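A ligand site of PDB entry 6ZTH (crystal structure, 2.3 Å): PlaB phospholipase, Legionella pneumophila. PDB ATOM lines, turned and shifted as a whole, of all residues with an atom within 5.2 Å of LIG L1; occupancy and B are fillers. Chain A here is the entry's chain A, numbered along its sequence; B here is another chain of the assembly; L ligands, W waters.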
ATOM      1  N   GLN A 140     -19.640   9.027  -4.990  1.00  0.00           N
ATOM      2  CA  GLN A 140     -19.423  10.339  -4.387  1.00  0.00           C
ATOM      3  C   GLN A 140     -19.820  11.485  -5.310  1.00  0.00           C
ATOM      4  O   GLN A 140     -20.051  12.596  -4.836  1.00  0.00           O
ATOM      5  CB  GLN A 140     -17.948  10.488  -3.988  1.00  0.00           C
ATOM      6  CG  GLN A 140     -17.602  11.830  -3.362  1.00  0.00           C
ATOM      7  CD  GLN A 140     -16.234  11.817  -2.697  1.00  0.00           C
ATOM      8  OE1 GLN A 140     -15.269  12.344  -3.239  1.00  0.00           O
ATOM      9  NE2 GLN A 140     -16.160  11.223  -1.516  1.00  0.00           N
ATOM     10  N   LEU A 141     -19.922  11.235  -6.626  1.00  0.00           N
ATOM     11  CA  LEU A 141     -20.241  12.303  -7.550  1.00  0.00           C
ATOM     12  C   LEU A 141     -21.622  12.897  -7.298  1.00  0.00           C
ATOM     13  O   LEU A 141     -21.873  14.050  -7.685  1.00  0.00           O
ATOM     14  CB  LEU A 141     -20.168  11.792  -8.988  1.00  0.00           C
ATOM     15  CG  LEU A 141     -18.776  11.534  -9.560  1.00  0.00           C
ATOM     16  CD1 LEU A 141     -18.879  11.019 -10.992  1.00  0.00           C
ATOM     17  CD2 LEU A 141     -17.899  12.774  -9.528  1.00  0.00           C
ATOM     18  N   ARG A 145     -25.845  14.540 -10.507  1.00  0.00           N
ATOM     19  CA  ARG A 145     -24.776  14.487 -11.496  1.00  0.00           C
ATOM     20  C   ARG A 145     -24.660  13.105 -12.107  1.00  0.00           C
ATOM     21  O   ARG A 145     -24.321  12.986 -13.293  1.00  0.00           O
ATOM     22  CB  ARG A 145     -23.454  14.911 -10.853  1.00  0.00           C
ATOM     23  CG  ARG A 145     -23.503  16.293 -10.207  1.00  0.00           C
ATOM     24  CD  ARG A 145     -22.314  17.158 -10.585  1.00  0.00           C
ATOM     25  NE  ARG A 145     -21.133  16.903  -9.764  1.00  0.00           N
ATOM     26  CZ  ARG A 145     -20.161  16.042 -10.084  1.00  0.00           C
ATOM     27  NH1 ARG A 145     -20.214  15.354 -11.221  1.00  0.00           N
ATOM     28  NH2 ARG A 145     -19.129  15.874  -9.262  1.00  0.00           N
ATOM     29  N   VAL A 208     -16.469  15.066 -18.685  1.00  0.00           N
ATOM     30  CA  VAL A 208     -16.017  15.815 -17.514  1.00  0.00           C
ATOM     31  C   VAL A 208     -15.966  14.929 -16.276  1.00  0.00           C
ATOM     32  O   VAL A 208     -15.984  15.438 -15.143  1.00  0.00           O
ATOM     33  CB  VAL A 208     -16.924  17.042 -17.265  1.00  0.00           C
ATOM     34  CG1 VAL A 208     -17.025  17.893 -18.521  1.00  0.00           C
ATOM     35  CG2 VAL A 208     -18.299  16.592 -16.797  1.00  0.00           C
ATOM     36  N   ASN A 209     -15.899  13.623 -16.475  1.00  0.00           N
ATOM     37  CA  ASN A 209     -15.765  12.669 -15.359  1.00  0.00           C
ATOM     38  C   ASN A 209     -14.882  11.524 -15.843  1.00  0.00           C
ATOM     39  O   ASN A 209     -15.339  10.653 -16.605  1.00  0.00           O
ATOM     40  CB  ASN A 209     -17.133  12.183 -14.894  1.00  0.00           C
ATOM     41  CG  ASN A 209     -17.852  13.192 -14.022  1.00  0.00           C
ATOM     42  OD1 ASN A 209     -17.262  13.766 -13.103  1.00  0.00           O
ATOM     43  ND2 ASN A 209     -19.122  13.426 -14.315  1.00  0.00           N
ATOM     44  N   SER A 210     -13.630  11.506 -15.396  1.00  0.00           N
ATOM     45  CA  SER A 210     -12.677  10.533 -15.887  1.00  0.00           C
ATOM     46  C   SER A 210     -12.978   9.116 -15.413  1.00  0.00           C
ATOM     47  O   SER A 210     -12.584   8.156 -16.077  1.00  0.00           O
ATOM     48  CB  SER A 210     -11.251  10.914 -15.464  1.00  0.00           C
ATOM     49  OG  SER A 210     -10.983  10.455 -14.147  1.00  0.00           O
ATOM     50  N   TYR A 211     -13.683   8.976 -14.286  1.00  0.00           N
ATOM     51  CA  TYR A 211     -13.960   7.642 -13.772  1.00  0.00           C
ATOM     52  C   TYR A 211     -14.658   6.776 -14.824  1.00  0.00           C
ATOM     53  O   TYR A 211     -14.472   5.556 -14.845  1.00  0.00           O
ATOM     54  CB  TYR A 211     -14.840   7.720 -12.515  1.00  0.00           C
ATOM     55  CG  TYR A 211     -14.111   8.133 -11.249  1.00  0.00           C
ATOM     56  CD1 TYR A 211     -12.788   7.772 -11.017  1.00  0.00           C
ATOM     57  CD2 TYR A 211     -14.764   8.861 -10.266  1.00  0.00           C
ATOM     58  CE1 TYR A 211     -12.130   8.148  -9.847  1.00  0.00           C
ATOM     59  CE2 TYR A 211     -14.127   9.234  -9.101  1.00  0.00           C
ATOM     60  CZ  TYR A 211     -12.814   8.880  -8.897  1.00  0.00           C
ATOM     61  OH  TYR A 211     -12.177   9.261  -7.736  1.00  0.00           O
ATOM     62  N   THR A 212     -15.454   7.391 -15.695  1.00  0.00           N
ATOM     63  CA  THR A 212     -16.199   6.641 -16.705  1.00  0.00           C
ATOM     64  C   THR A 212     -15.305   6.039 -17.787  1.00  0.00           C
ATOM     65  O   THR A 212     -15.832   5.404 -18.716  1.00  0.00           O
ATOM     66  CB  THR A 212     -17.263   7.532 -17.357  1.00  0.00           C
ATOM     67  OG1 THR A 212     -16.643   8.455 -18.246  1.00  0.00           O
ATOM     68  CG2 THR A 212     -18.046   8.300 -16.297  1.00  0.00           C
ATOM     69  N   ASP A 380      -5.467   7.329  -8.256  1.00  0.00           N
ATOM     70  CA  ASP A 380      -6.545   8.108  -7.651  1.00  0.00           C
ATOM     71  C   ASP A 380      -6.612   7.917  -6.146  1.00  0.00           C
ATOM     72  O   ASP A 380      -6.238   6.858  -5.626  1.00  0.00           O
ATOM     73  CB  ASP A 380      -7.881   7.733  -8.288  1.00  0.00           C
ATOM     74  CG  ASP A 380      -9.063   8.170  -7.467  1.00  0.00           C
ATOM     75  OD1 ASP A 380      -9.441   9.358  -7.545  1.00  0.00           O
ATOM     76  OD2 ASP A 380      -9.623   7.325  -6.726  1.00  0.00           O
ATOM     77  N   ARG A 381      -7.087   8.929  -5.425  1.00  0.00           N
ATOM     78  CA  ARG A 381      -7.460   8.798  -4.032  1.00  0.00           C
ATOM     79  C   ARG A 381      -8.794   9.497  -3.821  1.00  0.00           C
ATOM     80  O   ARG A 381      -9.109  10.478  -4.497  1.00  0.00           O
ATOM     81  CB  ARG A 381      -6.407   9.364  -3.083  1.00  0.00           C
ATOM     82  CG  ARG A 381      -6.225  10.873  -3.152  1.00  0.00           C
ATOM     83  CD  ARG A 381      -4.749  11.226  -3.119  1.00  0.00           C
ATOM     84  NE  ARG A 381      -4.503  12.660  -3.082  1.00  0.00           N
ATOM     85  CZ  ARG A 381      -3.430  13.224  -2.537  1.00  0.00           C
ATOM     86  NH1 ARG A 381      -3.286  14.541  -2.555  1.00  0.00           N
ATOM     87  NH2 ARG A 381      -2.492  12.467  -1.962  1.00  0.00           N
ATOM     88  N   GLN A 382      -9.574   8.983  -2.873  1.00  0.00           N
ATOM     89  CA  GLN A 382     -10.886   9.518  -2.567  1.00  0.00           C
ATOM     90  C   GLN A 382     -11.088   9.511  -1.054  1.00  0.00           C
ATOM     91  O   GLN A 382     -10.745   8.538  -0.385  1.00  0.00           O
ATOM     92  CB  GLN A 382     -11.989   8.691  -3.244  1.00  0.00           C
ATOM     93  CG  GLN A 382     -13.070   9.528  -3.929  1.00  0.00           C
ATOM     94  CD  GLN A 382     -14.231   8.686  -4.428  1.00  0.00           C
ATOM     95  OE1 GLN A 382     -14.917   8.019  -3.651  1.00  0.00           O
ATOM     96  NE2 GLN A 382     -14.455   8.710  -5.740  1.00  0.00           N
ATOM     97  N   TYR B 358     -23.771  23.091 -13.886  1.00  0.00           N
ATOM     98  CA  TYR B 358     -23.564  23.084 -15.325  1.00  0.00           C
ATOM     99  C   TYR B 358     -22.394  22.165 -15.642  1.00  0.00           C
ATOM    100  O   TYR B 358     -21.570  21.853 -14.770  1.00  0.00           O
ATOM    101  CB  TYR B 358     -23.281  24.505 -15.850  1.00  0.00           C
ATOM    102  CG  TYR B 358     -22.047  25.137 -15.241  1.00  0.00           C
ATOM    103  CD1 TYR B 358     -20.773  24.793 -15.672  1.00  0.00           C
ATOM    104  CD2 TYR B 358     -22.160  26.073 -14.221  1.00  0.00           C
ATOM    105  CE1 TYR B 358     -19.649  25.368 -15.112  1.00  0.00           C
ATOM    106  CE2 TYR B 358     -21.043  26.652 -13.655  1.00  0.00           C
ATOM    107  CZ  TYR B 358     -19.785  26.294 -14.109  1.00  0.00           C
ATOM    108  OH  TYR B 358     -18.668  26.865 -13.554  1.00  0.00           O
ATOM    109  N   ASP B 359     -22.314  21.757 -16.903  1.00  0.00           N
ATOM    110  CA  ASP B 359     -21.174  21.046 -17.438  1.00  0.00           C
ATOM    111  C   ASP B 359     -20.495  21.910 -18.493  1.00  0.00           C
ATOM    112  O   ASP B 359     -21.160  22.545 -19.319  1.00  0.00           O
ATOM    113  CB  ASP B 359     -21.576  19.702 -18.042  1.00  0.00           C
ATOM    114  CG  ASP B 359     -22.144  18.752 -17.025  1.00  0.00           C
ATOM    115  OD1 ASP B 359     -23.330  18.908 -16.663  1.00  0.00           O
ATOM    116  OD2 ASP B 359     -21.405  17.852 -16.559  1.00  0.00           O
ATOM    117  N   LEU B 360     -19.167  21.931 -18.461  1.00  0.00           N
ATOM    118  CA  LEU B 360     -18.357  22.721 -19.375  1.00  0.00           C
ATOM    119  C   LEU B 360     -17.463  21.787 -20.173  1.00  0.00           C
ATOM    120  O   LEU B 360     -16.924  20.820 -19.628  1.00  0.00           O
ATOM    121  CB  LEU B 360     -17.526  23.751 -18.626  1.00  0.00           C
ATOM    122  CG  LEU B 360     -16.636  24.632 -19.510  1.00  0.00           C
ATOM    123  CD1 LEU B 360     -17.455  25.702 -20.194  1.00  0.00           C
ATOM    124  CD2 LEU B 360     -15.541  25.244 -18.666  1.00  0.00           C
ATOM    125  N   TYR B 361     -17.309  22.090 -21.454  1.00  0.00           N
ATOM    126  CA  TYR B 361     -16.536  21.248 -22.362  1.00  0.00           C
ATOM    127  C   TYR B 361     -15.592  22.111 -23.181  1.00  0.00           C
ATOM    128  O   TYR B 361     -15.996  23.146 -23.719  1.00  0.00           O
ATOM    129  CB  TYR B 361     -17.453  20.463 -23.298  1.00  0.00           C
ATOM    130  CG  TYR B 361     -18.434  19.538 -22.604  1.00  0.00           C
ATOM    131  CD1 TYR B 361     -18.042  18.299 -22.136  1.00  0.00           C
ATOM    132  CD2 TYR B 361     -19.763  19.916 -22.427  1.00  0.00           C
ATOM    133  CE1 TYR B 361     -18.936  17.457 -21.504  1.00  0.00           C
ATOM    134  CE2 TYR B 361     -20.664  19.077 -21.789  1.00  0.00           C
ATOM    135  CZ  TYR B 361     -20.243  17.847 -21.328  1.00  0.00           C
ATOM    136  OH  TYR B 361     -21.131  17.010 -20.708  1.00  0.00           O
ATOM    137  N   ARG B 381      -7.989  21.008 -12.713  1.00  0.00           N
ATOM    138  CA  ARG B 381      -9.257  21.717 -12.669  1.00  0.00           C
ATOM    139  C   ARG B 381      -9.535  22.059 -11.207  1.00  0.00           C
ATOM    140  O   ARG B 381      -9.212  21.275 -10.310  1.00  0.00           O
ATOM    141  CB  ARG B 381     -10.403  20.877 -13.244  1.00  0.00           C
ATOM    142  CG  ARG B 381     -10.395  19.414 -12.814  1.00  0.00           C
ATOM    143  CD  ARG B 381     -11.193  18.520 -13.769  1.00  0.00           C
ATOM    144  NE  ARG B 381     -12.467  18.097 -13.183  1.00  0.00           N
ATOM    145  CZ  ARG B 381     -13.254  17.169 -13.700  1.00  0.00           C
ATOM    146  NH1 ARG B 381     -12.916  16.548 -14.830  1.00  0.00           N
ATOM    147  NH2 ARG B 381     -14.393  16.862 -13.103  1.00  0.00           N
ATOM    148  N   GLN B 382     -10.124  23.233 -10.974  1.00  0.00           N
ATOM    149  CA  GLN B 382     -10.430  23.662  -9.619  1.00  0.00           C
ATOM    150  C   GLN B 382     -11.745  24.433  -9.624  1.00  0.00           C
ATOM    151  O   GLN B 382     -12.004  25.244 -10.517  1.00  0.00           O
ATOM    152  CB  GLN B 382      -9.313  24.550  -9.037  1.00  0.00           C
ATOM    153  CG  GLN B 382      -8.500  23.890  -7.928  1.00  0.00           C
ATOM    154  CD  GLN B 382      -7.779  24.898  -7.051  1.00  0.00           C
ATOM    155  OE1 GLN B 382      -8.300  25.972  -6.756  1.00  0.00           O
ATOM    156  NE2 GLN B 382      -6.563  24.550  -6.629  1.00  0.00           N
ATOM    157  N   ARG B 383     -12.556  24.179  -8.605  1.00  0.00           N
ATOM    158  CA  ARG B 383     -13.841  24.859  -8.411  1.00  0.00           C
ATOM    159  C   ARG B 383     -13.745  25.713  -7.153  1.00  0.00           C
ATOM    160  O   ARG B 383     -13.445  25.197  -6.075  1.00  0.00           O
ATOM    161  CB  ARG B 383     -14.971  23.841  -8.300  1.00  0.00           C
ATOM    162  CG  ARG B 383     -16.209  24.178  -9.116  1.00  0.00           C
ATOM    163  CD  ARG B 383     -17.405  23.362  -8.634  1.00  0.00           C
ATOM    164  NE  ARG B 383     -18.636  23.667  -9.366  1.00  0.00           N
ATOM    165  CZ  ARG B 383     -19.806  23.082  -9.104  1.00  0.00           C
ATOM    166  NH1 ARG B 383     -20.887  23.413  -9.804  1.00  0.00           N
ATOM    167  NH2 ARG B 383     -19.903  22.180  -8.141  1.00  0.00           N
ATOM    168  N   LEU B 391     -14.901  28.294 -12.591  1.00  0.00           N
ATOM    169  CA  LEU B 391     -14.217  27.063 -12.986  1.00  0.00           C
ATOM    170  C   LEU B 391     -12.874  27.415 -13.600  1.00  0.00           C
ATOM    171  O   LEU B 391     -12.827  28.168 -14.578  1.00  0.00           O
ATOM    172  CB  LEU B 391     -15.081  26.275 -13.973  1.00  0.00           C
ATOM    173  CG  LEU B 391     -14.875  24.767 -14.032  1.00  0.00           C
ATOM    174  CD1 LEU B 391     -15.582  24.103 -12.870  1.00  0.00           C
ATOM    175  CD2 LEU B 391     -15.388  24.231 -15.348  1.00  0.00           C
ATOM    176  N   TYR B 393      -9.405  26.168 -15.374  1.00  0.00           N
ATOM    177  CA  TYR B 393      -8.698  25.146 -16.131  1.00  0.00           C
ATOM    178  C   TYR B 393      -7.198  25.402 -16.067  1.00  0.00           C
ATOM    179  O   TYR B 393      -6.747  26.554 -16.053  1.00  0.00           O
ATOM    180  CB  TYR B 393      -9.139  25.139 -17.598  1.00  0.00           C
ATOM    181  CG  TYR B 393     -10.448  24.431 -17.895  1.00  0.00           C
ATOM    182  CD1 TYR B 393     -10.938  23.428 -17.074  1.00  0.00           C
ATOM    183  CD2 TYR B 393     -11.177  24.757 -19.028  1.00  0.00           C
ATOM    184  CE1 TYR B 393     -12.127  22.788 -17.362  1.00  0.00           C
ATOM    185  CE2 TYR B 393     -12.360  24.123 -19.327  1.00  0.00           C
ATOM    186  CZ  TYR B 393     -12.828  23.130 -18.490  1.00  0.00           C
ATOM    187  OH  TYR B 393     -14.010  22.496 -18.790  1.00  0.00           O
HETATM  188  P1  LIG L   1     -12.798  17.628  -8.795  1.00  0.00           P
HETATM  189  O1  LIG L   1     -11.774  18.338  -7.954  1.00  0.00           O
HETATM  190  O2  LIG L   1     -12.167  17.130 -10.076  1.00  0.00           O
HETATM  191  O3  LIG L   1     -14.011  18.659  -9.157  1.00  0.00           O
HETATM  192  C1  LIG L   1     -14.356  19.642  -8.198  1.00  0.00           C
HETATM  193  C2  LIG L   1     -15.754  20.291  -8.586  1.00  0.00           C
HETATM  194  O4  LIG L   1     -15.579  21.051  -9.939  1.00  0.00           O
HETATM  195  C3  LIG L   1     -16.637  19.404  -8.767  1.00  0.00           C
HETATM  196  O5  LIG L   1     -17.907  19.837  -8.183  1.00  0.00           O
HETATM  197  C4  LIG L   1     -16.814  19.244 -10.418  1.00  0.00           C
HETATM  198  O6  LIG L   1     -18.142  18.738 -10.765  1.00  0.00           O
HETATM  199  C5  LIG L   1     -16.651  20.438 -10.866  1.00  0.00           C
HETATM  200  N1  LIG L   1     -16.197  20.426 -12.313  1.00  0.00           N
HETATM  201  C6  LIG L   1     -14.976  19.968 -12.599  1.00  0.00           C
HETATM  202  N2  LIG L   1     -14.804  20.058 -13.928  1.00  0.00           N
HETATM  203  C7  LIG L   1     -15.936  20.566 -14.458  1.00  0.00           C
HETATM  204  C8  LIG L   1     -16.301  20.868 -15.759  1.00  0.00           C
HETATM  205  N3  LIG L   1     -15.564  20.718 -17.029  1.00  0.00           N
HETATM  206  N4  LIG L   1     -17.491  21.382 -16.016  1.00  0.00           N
HETATM  207  C9  LIG L   1     -18.367  21.616 -14.991  1.00  0.00           C
HETATM  208  N5  LIG L   1     -18.017  21.324 -13.711  1.00  0.00           N
HETATM  209  C10 LIG L   1     -16.799  20.810 -13.456  1.00  0.00           C
HETATM  210  O7  LIG L   1     -13.420  16.340  -7.955  1.00  0.00           O
HETATM  211  P2  LIG L   1     -14.798  15.564  -8.404  1.00  0.00           P
HETATM  212  O8  LIG L   1     -14.886  15.542  -9.904  1.00  0.00           O
HETATM  213  O9  LIG L   1     -16.007  16.298  -7.845  1.00  0.00           O
HETATM  214  O10 LIG L   1     -14.756  14.016  -7.803  1.00  0.00           O
HETATM  215  C11 LIG L   1     -14.696  13.829  -6.400  1.00  0.00           C
HETATM  216  C12 LIG L   1     -13.468  13.002  -6.027  1.00  0.00           C
HETATM  217  O11 LIG L   1     -13.279  12.038  -6.880  1.00  0.00           O
HETATM  218  C13 LIG L   1     -12.118  13.954  -6.049  1.00  0.00           C
HETATM  219  O12 LIG L   1     -11.194  13.501  -4.971  1.00  0.00           O
HETATM  220  C14 LIG L   1     -11.589  13.786  -7.154  1.00  0.00           C
HETATM  221  O13 LIG L   1     -10.096  14.029  -7.092  1.00  0.00           O
HETATM  222  C15 LIG L   1     -11.904  12.248  -7.462  1.00  0.00           C
HETATM  223  N6  LIG L   1     -11.915  12.010  -8.784  1.00  0.00           N
HETATM  224  C16 LIG L   1     -13.040  12.213  -9.520  1.00  0.00           C
HETATM  225  C17 LIG L   1     -13.040  11.946 -10.892  1.00  0.00           C
HETATM  226  C18 LIG L   1     -14.323  12.172 -11.754  1.00  0.00           C
HETATM  227  O14 LIG L   1     -14.622  11.385 -12.585  1.00  0.00           O
HETATM  228  N7  LIG L   1     -15.169  13.366 -11.548  1.00  0.00           N
HETATM  229  C19 LIG L   1     -11.892  11.495 -11.497  1.00  0.00           C
HETATM  230  C20 LIG L   1     -10.767  11.292 -10.761  1.00  0.00           C
HETATM  231  C21 LIG L   1     -10.780  11.550  -9.383  1.00  0.00           C
HETATM  232  P1  LG2 L   2      -8.434  15.494  -3.199  1.00  0.00           P
HETATM  233  O1  LG2 L   2      -9.591  14.856  -3.925  1.00  0.00           O
HETATM  234  O2  LG2 L   2      -7.136  14.997  -3.796  1.00  0.00           O
HETATM  235  O3  LG2 L   2      -8.494  15.083  -1.615  1.00  0.00           O
HETATM  236  C1  LG2 L   2      -9.776  14.933  -1.017  1.00  0.00           C
HETATM  237  C2  LG2 L   2      -9.618  15.050   0.562  1.00  0.00           C
HETATM  238  O4  LG2 L   2      -8.833  13.803   1.065  1.00  0.00           O
HETATM  239  C3  LG2 L   2      -8.932  16.062   0.873  1.00  0.00           C
HETATM  240  O5  LG2 L   2      -9.432  16.648   2.117  1.00  0.00           O
HETATM  241  C4  LG2 L   2      -7.369  15.521   1.095  1.00  0.00           C
HETATM  242  O6  LG2 L   2      -6.633  16.429   1.980  1.00  0.00           O
HETATM  243  C5  LG2 L   2      -7.516  14.370   1.657  1.00  0.00           C
HETATM  244  N1  LG2 L   2      -6.356  13.440   1.380  1.00  0.00           N
HETATM  245  C6  LG2 L   2      -6.072  13.103   0.104  1.00  0.00           C
HETATM  246  N2  LG2 L   2      -5.004  12.286   0.130  1.00  0.00           N
HETATM  247  C7  LG2 L   2      -4.640  12.116   1.419  1.00  0.00           C
HETATM  248  C8  LG2 L   2      -3.618  11.374   1.994  1.00  0.00           C
HETATM  249  N3  LG2 L   2      -2.574  10.517   1.396  1.00  0.00           N
HETATM  250  N4  LG2 L   2      -3.479  11.374   3.315  1.00  0.00           N
HETATM  251  C9  LG2 L   2      -4.332  12.097   4.085  1.00  0.00           C
HETATM  252  N5  LG2 L   2      -5.333  12.825   3.524  1.00  0.00           N
HETATM  253  C10 LG2 L   2      -5.473  12.826   2.186  1.00  0.00           C
HETATM  254  O7  LG2 L   2      -8.527  17.142  -3.346  1.00  0.00           O
HETATM  255  P2  LG2 L   2      -7.569  18.185  -2.506  1.00  0.00           P
HETATM  256  O8  LG2 L   2      -6.235  17.538  -2.230  1.00  0.00           O
HETATM  257  O9  LG2 L   2      -8.239  18.541  -1.188  1.00  0.00           O
HETATM  258  O10 LG2 L   2      -7.355  19.557  -3.408  1.00  0.00           O
HETATM  259  C11 LG2 L   2      -8.485  20.357  -3.697  1.00  0.00           C
HETATM  260  C12 LG2 L   2      -8.638  20.537  -5.204  1.00  0.00           C
HETATM  261  O11 LG2 L   2      -7.465  20.779  -5.734  1.00  0.00           O
HETATM  262  C13 LG2 L   2      -9.210  19.149  -5.910  1.00  0.00           C
HETATM  263  O12 LG2 L   2     -10.102  19.512  -7.045  1.00  0.00           O
HETATM  264  C14 LG2 L   2      -8.225  18.539  -6.338  1.00  0.00           C
HETATM  265  O13 LG2 L   2      -8.594  17.685  -7.535  1.00  0.00           O
HETATM  266  C15 LG2 L   2      -7.239  19.704  -6.762  1.00  0.00           C
HETATM  267  N6  LG2 L   2      -5.952  19.316  -6.733  1.00  0.00           N
HETATM  268  C16 LG2 L   2      -5.244  19.402  -5.569  1.00  0.00           C
HETATM  269  C17 LG2 L   2      -3.900  19.005  -5.539  1.00  0.00           C
HETATM  270  C18 LG2 L   2      -3.094  19.100  -4.207  1.00  0.00           C
HETATM  271  O14 LG2 L   2      -1.983  19.486  -4.209  1.00  0.00           O
HETATM  272  N7  LG2 L   2      -3.730  18.717  -2.927  1.00  0.00           N
HETATM  273  C19 LG2 L   2      -3.308  18.523  -6.670  1.00  0.00           C
HETATM  274  C20 LG2 L   2      -4.017  18.438  -7.834  1.00  0.00           C
HETATM  275  C21 LG2 L   2      -5.367  18.838  -7.858  1.00  0.00           C
HETATM  276  P1  LG3 L   3      -8.769  12.478 -19.572  1.00  0.00           P
HETATM  277  O1  LG3 L   3      -9.829  11.998 -20.512  1.00  0.00           O
HETATM  278  O2  LG3 L   3      -8.464  11.413 -18.542  1.00  0.00           O
HETATM  279  O3  LG3 L   3      -9.292  13.836 -18.812  1.00  0.00           O
HETATM  280  C1  LG3 L   3      -8.512  14.309 -17.724  1.00  0.00           C
HETATM  281  C2  LG3 L   3      -9.384  15.351 -16.901  1.00  0.00           C
HETATM  282  O4  LG3 L   3      -9.984  16.390 -17.895  1.00  0.00           O
HETATM  283  C3  LG3 L   3     -10.377  14.791 -16.354  1.00  0.00           C
HETATM  284  O5  LG3 L   3     -10.707  15.500 -15.112  1.00  0.00           O
HETATM  285  C4  LG3 L   3     -11.634  14.922 -17.442  1.00  0.00           C
HETATM  286  O6  LG3 L   3     -12.915  14.840 -16.728  1.00  0.00           O
HETATM  287  C5  LG3 L   3     -11.532  16.071 -17.942  1.00  0.00           C
HETATM  288  N1  LG3 L   3     -11.986  16.218 -19.384  1.00  0.00           N
HETATM  289  C6  LG3 L   3     -11.667  15.304 -20.300  1.00  0.00           C
HETATM  290  N2  LG3 L   3     -12.193  15.695 -21.477  1.00  0.00           N
HETATM  291  C7  LG3 L   3     -12.835  16.860 -21.276  1.00  0.00           C
HETATM  292  C8  LG3 L   3     -13.531  17.703 -22.140  1.00  0.00           C
HETATM  293  N3  LG3 L   3     -13.821  17.567 -23.583  1.00  0.00           N
HETATM  294  N4  LG3 L   3     -14.075  18.816 -21.678  1.00  0.00           N
HETATM  295  C9  LG3 L   3     -13.931  19.149 -20.364  1.00  0.00           C
HETATM  296  N5  LG3 L   3     -13.250  18.340 -19.520  1.00  0.00           N
HETATM  297  C10 LG3 L   3     -12.699  17.199 -19.990  1.00  0.00           C
HETATM  298  O7  LG3 L   3      -7.392  12.853 -20.408  1.00  0.00           O
HETATM  299  P2  LG3 L   3      -7.124  12.498 -21.992  1.00  0.00           P
HETATM  300  O8  LG3 L   3      -7.061  11.005 -22.173  1.00  0.00           O
HETATM  301  O9  LG3 L   3      -5.803  13.117 -22.424  1.00  0.00           O
HETATM  302  O10 LG3 L   3      -8.342  13.131 -22.917  1.00  0.00           O
HETATM  303  C11 LG3 L   3      -8.089  13.308 -24.303  1.00  0.00           C
HETATM  304  C12 LG3 L   3      -9.391  13.131 -25.060  1.00  0.00           C
HETATM  305  O11 LG3 L   3      -9.679  11.863 -25.166  1.00  0.00           O
HETATM  306  C13 LG3 L   3     -10.622  13.849 -24.210  1.00  0.00           C
HETATM  307  O12 LG3 L   3     -11.523  14.561 -25.163  1.00  0.00           O
HETATM  308  C14 LG3 L   3     -11.244  12.940 -23.633  1.00  0.00           C
HETATM  309  O13 LG3 L   3     -12.704  13.324 -23.516  1.00  0.00           O
HETATM  310  C15 LG3 L   3     -11.062  11.683 -24.592  1.00  0.00           C
HETATM  311  N6  LG3 L   3     -11.138  10.504 -23.945  1.00  0.00           N
HETATM  312  C16 LG3 L   3     -12.040   9.582 -24.383  1.00  0.00           C
HETATM  313  C17 LG3 L   3     -12.144   8.337 -23.728  1.00  0.00           C
HETATM  314  C18 LG3 L   3     -13.185   7.287 -24.237  1.00  0.00           C
HETATM  315  O14 LG3 L   3     -13.118   6.176 -23.862  1.00  0.00           O
HETATM  316  N7  LG3 L   3     -14.228   7.673 -25.202  1.00  0.00           N
HETATM  317  C19 LG3 L   3     -11.342   8.054 -22.667  1.00  0.00           C
HETATM  318  C20 LG3 L   3     -10.442   8.985 -22.234  1.00  0.00           C
HETATM  319  C21 LG3 L   3     -10.337  10.221 -22.884  1.00  0.00           C
HETATM  320  O   HOH W   1      -7.373  12.452  -7.149  1.00  0.00           O
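The backbone NH (N) of Asn 209 sits at hydrogen-bond distance from an oxygen (O6) of LG3 L3.
The side-chain amide oxygen (OD1) of Asn 209 is in hydrogen-bond range of a nitrogen (N7) of LIG L1 (2.6 Å).
The backbone carbonyl oxygen of Leu 360 of chain B lies within hydrogen-bond range of a nitrogen (N3) of LIG L1, 2.9 Å away.
The side-chain hydroxyl (OH) of Tyr 211 lies close to an oxygen (O11) of LIG L1 (3.1 Å).
The backbone NH of Ser 210 sits at hydrogen-bond distance from an oxygen (O14) of LIG L1, at 3.0 Å.
NE of Arg 381 of chain B is in salt-bridge range of O2 of LIG L1, at 3.3 Å.
The backbone NH (N) of Tyr 211 lies within hydrogen-bond range of an oxygen (O14) of LIG L1 (3.1 Å).
NE of Arg 381 of chain A is in salt-bridge range of O2 of LG2 L2 (3.6 Å).
NH1 of Arg 381 of chain B is in hydrogen-bond range of O5 of LG3 L3 (2.5 Å).
An oxygen (O9) of LIG L1 lies within salt-bridge range of the guanidinium group (NH2) of Arg 145 (3.5 Å).
The guanidinium group (NH2) of Arg 383 of chain B lies within hydrogen-bond range of an oxygen (O5) of LIG L1 (3.1 Å).
A nitrogen (N3) of LIG L1 lies within hydrogen-bond range of the side-chain hydroxyl of Tyr 393 of chain B (2.9 Å).
A nitrogen (N4) of LIG L1 sits at hydrogen-bond distance from the backbone NH (N) of Leu 360 of chain B, at 3.0 Å.
O1 of LIG L1 lies within hydrogen-bond range of O13 of LG2 L2 (3.3 Å).
The guanidinium group (NH2) of Arg 381 of chain B lies within hydrogen-bond range of the backbone carbonyl oxygen (O) of Val 208, 3.0 Å away.
The backbone carbonyl oxygen (O) of Asn 209 is in hydrogen-bond range of the side-chain hydroxyl (OG1) of Thr 212, at 3.0 Å.
The backbone carbonyl oxygen of Leu 360 of chain B lies close to the side-chain hydroxyl of Tyr 393 of chain B (3.5 Å).
The side-chain hydroxyl of Tyr 211 is in hydrogen-bond range of the side-chain amide nitrogen of Gln 382 of chain A, 3.1 Å away.
OH of Tyr 211 lies within hydrogen-bond range of OD1 of Asp 380, 2.7 Å away.
Merely in contact with LIG L1: Gln 140, Leu 141, Val 208, Asp 380, Arg 381 of chain A, Gln 382 of chain A, Tyr 358 of chain B, Asp 359 of chain B and Leu 391 of chain B.
The nearest printed residue that does not touch LIG L1 is Tyr 361 of chain B (5.0 Å).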
